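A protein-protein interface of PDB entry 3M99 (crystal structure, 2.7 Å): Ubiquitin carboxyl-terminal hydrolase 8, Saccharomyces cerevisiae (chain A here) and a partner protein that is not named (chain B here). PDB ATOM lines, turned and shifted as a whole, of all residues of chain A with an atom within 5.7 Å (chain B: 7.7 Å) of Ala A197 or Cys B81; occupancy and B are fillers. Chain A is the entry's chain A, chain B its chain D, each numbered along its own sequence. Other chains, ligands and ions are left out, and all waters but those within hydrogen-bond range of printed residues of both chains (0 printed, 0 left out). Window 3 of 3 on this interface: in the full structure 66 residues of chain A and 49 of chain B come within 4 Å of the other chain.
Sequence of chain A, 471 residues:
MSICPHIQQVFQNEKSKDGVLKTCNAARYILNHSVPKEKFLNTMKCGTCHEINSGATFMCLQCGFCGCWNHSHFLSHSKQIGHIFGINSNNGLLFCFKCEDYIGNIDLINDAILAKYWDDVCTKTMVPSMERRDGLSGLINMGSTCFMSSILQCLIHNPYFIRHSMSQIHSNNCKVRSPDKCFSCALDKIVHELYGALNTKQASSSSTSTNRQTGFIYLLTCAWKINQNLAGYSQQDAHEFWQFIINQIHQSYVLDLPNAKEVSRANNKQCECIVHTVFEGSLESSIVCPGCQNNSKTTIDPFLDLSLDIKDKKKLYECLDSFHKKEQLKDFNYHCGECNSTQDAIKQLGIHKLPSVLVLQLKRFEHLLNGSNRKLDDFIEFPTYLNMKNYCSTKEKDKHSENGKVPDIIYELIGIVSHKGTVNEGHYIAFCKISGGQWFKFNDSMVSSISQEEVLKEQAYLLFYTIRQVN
A ring nitrogen (NE2) of His A192 sits at hydrogen-bond distance from the backbone carbonyl oxygen (O) of Cys B81 (3.1 Å).
N of Ala A197 is in hydrogen-bond range of O of Gly B82 (3.2 Å).
The backbone carbonyl oxygen of Ala A197 sits close to the backbone carbonyl oxygen of Cys B81.
N of Cys B78 is in hydrogen-bond range of O of Lys B83 (3.0 Å).
The side-chain sulfur of Cys B81 sits close to the backbone NH of Lys B83 (3.2 Å).
Among the printed residues, merely in contact across the chains: His A192 with Gly B82 (3.7 Å), His A192 with Lys B83 (3.5 Å), His A192 with Pro B84 (3.6 Å), Tyr A195 with Val B77 (3.9 Å), Tyr A195 with Pro B84 (3.5 Å), Gly A196 with Gly B82 (3.6 Å) and Gly A196 with Pro B84 (3.7 Å).
Ala A197 touches two residues of chain B.
Of chain A, only His A192 (3.1 Å) and Ala A197 (3.2 Å) come within 4 Å of Cys B81.
Of chain B, only Gly B82 (3.6 Å) and Pro B84 (3.7 Å) come within 4 Å of Gly A196.
Of the printed residues of chain A, Gly B82 touches His A192, Gly A196 and Ala A197.
Printed residues of chain A within 4 Å of Lys B83: His A192 (3.5 Å).
Of the printed residues of chain B, Tyr A195 touches Val B77 (3.9 Å) and Pro B84 (3.5 Å).
Lys B80 touches none of the printed residues of chain A.
Glu B79 touches none of the printed residues of chain A.
The nearest residue of chain B that does not touch Ala A197 is Lys B83 (4.4 Å).
The nearest residue of chain A that does not touch Cys B81 is Leu A198 (4.1 Å).
Of the 12 printed residues of chain B, 5 touch a printed residue of chain A.
Printed residues of chain B that touch a printed residue of chain A: Val B77, Cys B81, Gly B82, Lys B83 and Pro B84.
Hydrophobic or aromatic side chains of chain A that line the printed part of chain B: His A192 and Tyr A195.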
ATOM      1  N   HIS A 192       0.184 -26.118 -35.566  1.00  0.00           N
ATOM      2  CA  HIS A 192      -0.114 -26.589 -34.222  1.00  0.00           C
ATOM      3  C   HIS A 192      -1.243 -27.629 -34.205  1.00  0.00           C
ATOM      4  O   HIS A 192      -1.082 -28.703 -33.641  1.00  0.00           O
ATOM      5  CB  HIS A 192      -0.463 -25.387 -33.347  1.00  0.00           C
ATOM      6  CG  HIS A 192      -0.855 -25.745 -31.947  1.00  0.00           C
ATOM      7  ND1 HIS A 192      -1.427 -26.947 -31.616  1.00  0.00           N
ATOM      8  CD2 HIS A 192      -0.790 -25.021 -30.802  1.00  0.00           C
ATOM      9  CE1 HIS A 192      -1.679 -26.968 -30.319  1.00  0.00           C
ATOM     10  NE2 HIS A 192      -1.308 -25.816 -29.803  1.00  0.00           N
ATOM     11  N   GLU A 193      -2.382 -27.320 -34.820  1.00  0.00           N
ATOM     12  CA  GLU A 193      -3.500 -28.265 -34.865  1.00  0.00           C
ATOM     13  C   GLU A 193      -3.418 -29.178 -36.083  1.00  0.00           C
ATOM     14  O   GLU A 193      -4.433 -29.494 -36.701  1.00  0.00           O
ATOM     15  CB  GLU A 193      -4.840 -27.526 -34.911  1.00  0.00           C
ATOM     16  CG  GLU A 193      -5.231 -26.749 -33.658  1.00  0.00           C
ATOM     17  CD  GLU A 193      -6.499 -25.923 -33.880  1.00  0.00           C
ATOM     18  OE1 GLU A 193      -7.276 -26.258 -34.808  1.00  0.00           O
ATOM     19  OE2 GLU A 193      -6.715 -24.940 -33.133  1.00  0.00           O
ATOM     20  N   TYR A 195       0.016 -31.004 -36.515  1.00  0.00           N
ATOM     21  CA  TYR A 195       1.132 -31.840 -36.096  1.00  0.00           C
ATOM     22  C   TYR A 195       1.035 -32.137 -34.604  1.00  0.00           C
ATOM     23  O   TYR A 195       1.779 -32.966 -34.089  1.00  0.00           O
ATOM     24  CB  TYR A 195       2.466 -31.142 -36.384  1.00  0.00           C
ATOM     25  CG  TYR A 195       2.841 -31.071 -37.847  1.00  0.00           C
ATOM     26  CD1 TYR A 195       2.397 -30.033 -38.649  1.00  0.00           C
ATOM     27  CD2 TYR A 195       3.645 -32.039 -38.422  1.00  0.00           C
ATOM     28  CE1 TYR A 195       2.739 -29.968 -39.980  1.00  0.00           C
ATOM     29  CE2 TYR A 195       3.986 -31.980 -39.750  1.00  0.00           C
ATOM     30  CZ  TYR A 195       3.530 -30.942 -40.523  1.00  0.00           C
ATOM     31  OH  TYR A 195       3.869 -30.874 -41.849  1.00  0.00           O
ATOM     32  N   GLY A 196       0.128 -31.451 -33.913  1.00  0.00           N
ATOM     33  CA  GLY A 196      -0.042 -31.620 -32.479  1.00  0.00           C
ATOM     34  C   GLY A 196      -1.485 -31.588 -31.992  1.00  0.00           C
ATOM     35  O   GLY A 196      -2.396 -32.091 -32.659  1.00  0.00           O
ATOM     36  N   ALA A 197      -1.692 -30.983 -30.823  1.00  0.00           N
ATOM     37  CA  ALA A 197      -2.995 -30.983 -30.164  1.00  0.00           C
ATOM     38  C   ALA A 197      -3.319 -29.634 -29.507  1.00  0.00           C
ATOM     39  O   ALA A 197      -2.535 -29.121 -28.706  1.00  0.00           O
ATOM     40  CB  ALA A 197      -3.041 -32.094 -29.133  1.00  0.00           C
ATOM     41  N   LEU A 198      -4.475 -29.064 -29.847  1.00  0.00           N
ATOM     42  CA  LEU A 198      -4.946 -27.832 -29.206  1.00  0.00           C
ATOM     43  C   LEU A 198      -6.349 -27.992 -28.624  1.00  0.00           C
ATOM     44  O   LEU A 198      -6.911 -29.090 -28.610  1.00  0.00           O
ATOM     45  CB  LEU A 198      -4.927 -26.654 -30.185  1.00  0.00           C
ATOM     46  CG  LEU A 198      -5.054 -25.236 -29.599  1.00  0.00           C
ATOM     47  CD1 LEU A 198      -4.260 -25.079 -28.292  1.00  0.00           C
ATOM     48  CD2 LEU A 198      -4.652 -24.158 -30.620  1.00  0.00           C
ATOM     49  N   VAL B  77       5.904 -33.156 -29.096  1.00  0.00           N
ATOM     50  CA  VAL B  77       4.765 -32.335 -28.702  1.00  0.00           C
ATOM     51  C   VAL B  77       4.809 -31.993 -27.222  1.00  0.00           C
ATOM     52  O   VAL B  77       4.911 -32.879 -26.381  1.00  0.00           O
ATOM     53  CB  VAL B  77       3.442 -33.082 -28.980  1.00  0.00           C
ATOM     54  CG1 VAL B  77       2.255 -32.331 -28.391  1.00  0.00           C
ATOM     55  CG2 VAL B  77       3.267 -33.308 -30.468  1.00  0.00           C
ATOM     56  N   CYS B  78       4.717 -30.710 -26.899  1.00  0.00           N
ATOM     57  CA  CYS B  78       4.670 -30.297 -25.503  1.00  0.00           C
ATOM     58  C   CYS B  78       3.502 -30.944 -24.770  1.00  0.00           C
ATOM     59  O   CYS B  78       2.422 -31.126 -25.328  1.00  0.00           O
ATOM     60  CB  CYS B  78       4.569 -28.780 -25.379  1.00  0.00           C
ATOM     61  SG  CYS B  78       3.943 -28.225 -23.774  1.00  0.00           S
ATOM     62  N   GLU B  79       3.731 -31.273 -23.505  1.00  0.00           N
ATOM     63  CA  GLU B  79       2.730 -31.930 -22.681  1.00  0.00           C
ATOM     64  C   GLU B  79       1.469 -31.111 -22.426  1.00  0.00           C
ATOM     65  O   GLU B  79       0.372 -31.664 -22.384  1.00  0.00           O
ATOM     66  CB  GLU B  79       3.349 -32.350 -21.350  1.00  0.00           C
ATOM     67  CG  GLU B  79       3.795 -33.794 -21.333  1.00  0.00           C
ATOM     68  CD  GLU B  79       2.659 -34.739 -21.675  1.00  0.00           C
ATOM     69  OE1 GLU B  79       1.506 -34.450 -21.282  1.00  0.00           O
ATOM     70  OE2 GLU B  79       2.915 -35.767 -22.338  1.00  0.00           O
ATOM     71  N   LYS B  80       1.614 -29.802 -22.256  1.00  0.00           N
ATOM     72  CA  LYS B  80       0.489 -28.980 -21.811  1.00  0.00           C
ATOM     73  C   LYS B  80      -0.118 -28.039 -22.867  1.00  0.00           C
ATOM     74  O   LYS B  80      -1.332 -27.818 -22.880  1.00  0.00           O
ATOM     75  CB  LYS B  80       0.874 -28.214 -20.539  1.00  0.00           C
ATOM     76  CG  LYS B  80       1.207 -29.132 -19.363  1.00  0.00           C
ATOM     77  CD  LYS B  80       1.630 -28.354 -18.121  1.00  0.00           C
ATOM     78  CE  LYS B  80       1.674 -29.263 -16.894  1.00  0.00           C
ATOM     79  NZ  LYS B  80       2.105 -28.550 -15.652  1.00  0.00           N
ATOM     80  N   CYS B  81       0.711 -27.483 -23.745  1.00  0.00           N
ATOM     81  CA  CYS B  81       0.190 -26.608 -24.795  1.00  0.00           C
ATOM     82  C   CYS B  81      -0.081 -27.396 -26.076  1.00  0.00           C
ATOM     83  O   CYS B  81      -0.880 -26.983 -26.918  1.00  0.00           O
ATOM     84  CB  CYS B  81       1.127 -25.421 -25.055  1.00  0.00           C
ATOM     85  SG  CYS B  81       2.455 -25.718 -26.243  1.00  0.00           S
ATOM     86  N   GLY B  82       0.579 -28.541 -26.204  1.00  0.00           N
ATOM     87  CA  GLY B  82       0.378 -29.409 -27.349  1.00  0.00           C
ATOM     88  C   GLY B  82       1.021 -28.918 -28.633  1.00  0.00           C
ATOM     89  O   GLY B  82       0.897 -29.568 -29.666  1.00  0.00           O
ATOM     90  N   LYS B  83       1.696 -27.772 -28.581  1.00  0.00           N
ATOM     91  CA  LYS B  83       2.436 -27.288 -29.741  1.00  0.00           C
ATOM     92  C   LYS B  83       3.447 -28.346 -30.178  1.00  0.00           C
ATOM     93  O   LYS B  83       4.032 -29.032 -29.341  1.00  0.00           O
ATOM     94  CB  LYS B  83       3.188 -25.993 -29.413  1.00  0.00           C
ATOM     95  CG  LYS B  83       2.371 -24.711 -29.450  1.00  0.00           C
ATOM     96  CD  LYS B  83       3.174 -23.555 -28.855  1.00  0.00           C
ATOM     97  CE  LYS B  83       2.461 -22.218 -29.010  1.00  0.00           C
ATOM     98  NZ  LYS B  83       2.488 -21.720 -30.419  1.00  0.00           N
ATOM     99  N   PRO B  84       3.649 -28.488 -31.495  1.00  0.00           N
ATOM    100  CA  PRO B  84       4.725 -29.318 -32.049  1.00  0.00           C
ATOM    101  C   PRO B  84       6.064 -28.583 -31.999  1.00  0.00           C
ATOM    102  O   PRO B  84       6.302 -27.680 -32.802  1.00  0.00           O
ATOM    103  CB  PRO B  84       4.298 -29.520 -33.509  1.00  0.00           C
ATOM    104  CG  PRO B  84       2.888 -29.023 -33.597  1.00  0.00           C
ATOM    105  CD  PRO B  84       2.758 -27.982 -32.547  1.00  0.00           C
ATOM    106  N   LEU B  85       6.921 -28.976 -31.063  1.00  0.00           N
ATOM    107  CA  LEU B  85       8.211 -28.332 -30.857  1.00  0.00           C
ATOM    108  C   LEU B  85       9.281 -28.935 -31.740  1.00  0.00           C
ATOM    109  O   LEU B  85       9.315 -30.145 -31.944  1.00  0.00           O
ATOM    110  CB  LEU B  85       8.646 -28.481 -29.401  1.00  0.00           C
ATOM    111  CG  LEU B  85       7.612 -28.122 -28.338  1.00  0.00           C
ATOM    112  CD1 LEU B  85       8.104 -28.502 -26.953  1.00  0.00           C
ATOM    113  CD2 LEU B  85       7.294 -26.644 -28.401  1.00  0.00           C
ATOM    114  N   HIS B  93      11.590 -23.808 -24.670  1.00  0.00           N
ATOM    115  CA  HIS B  93      10.148 -23.649 -24.629  1.00  0.00           C
ATOM    116  C   HIS B  93       9.582 -24.109 -23.291  1.00  0.00           C
ATOM    117  O   HIS B  93       8.766 -23.419 -22.681  1.00  0.00           O
ATOM    118  CB  HIS B  93       9.497 -24.410 -25.783  1.00  0.00           C
ATOM    119  CG  HIS B  93       8.014 -24.526 -25.664  1.00  0.00           C
ATOM    120  ND1 HIS B  93       7.148 -23.566 -26.143  1.00  0.00           N
ATOM    121  CD2 HIS B  93       7.233 -25.488 -25.112  1.00  0.00           C
ATOM    122  CE1 HIS B  93       5.905 -23.932 -25.896  1.00  0.00           C
ATOM    123  NE2 HIS B  93       5.932 -25.096 -25.270  1.00  0.00           N
ATOM    124  N   HIS B  97       8.652 -20.310 -22.206  1.00  0.00           N
ATOM    125  CA  HIS B  97       7.603 -19.795 -23.083  1.00  0.00           C
ATOM    126  C   HIS B  97       6.241 -20.480 -23.034  1.00  0.00           C
ATOM    127  O   HIS B  97       5.235 -19.880 -23.412  1.00  0.00           O
ATOM    128  CB  HIS B  97       8.115 -19.774 -24.509  1.00  0.00           C
ATOM    129  CG  HIS B  97       9.145 -18.723 -24.744  1.00  0.00           C
ATOM    130  ND1 HIS B  97       9.164 -17.945 -25.879  1.00  0.00           N
ATOM    131  CD2 HIS B  97      10.171 -18.293 -23.974  1.00  0.00           C
ATOM    132  CE1 HIS B  97      10.173 -17.099 -25.810  1.00  0.00           C
ATOM    133  NE2 HIS B  97      10.801 -17.287 -24.662  1.00  0.00           N
ATOM    134  N   CYS B  98       6.200 -21.726 -22.582  1.00  0.00           N
ATOM    135  CA  CYS B  98       4.930 -22.437 -22.523  1.00  0.00           C
ATOM    136  C   CYS B  98       3.984 -21.803 -21.507  1.00  0.00           C
ATOM    137  O   CYS B  98       2.847 -21.460 -21.836  1.00  0.00           O
ATOM    138  CB  CYS B  98       5.137 -23.915 -22.200  1.00  0.00           C
ATOM    139  SG  CYS B  98       3.586 -24.809 -22.010  1.00  0.00           S
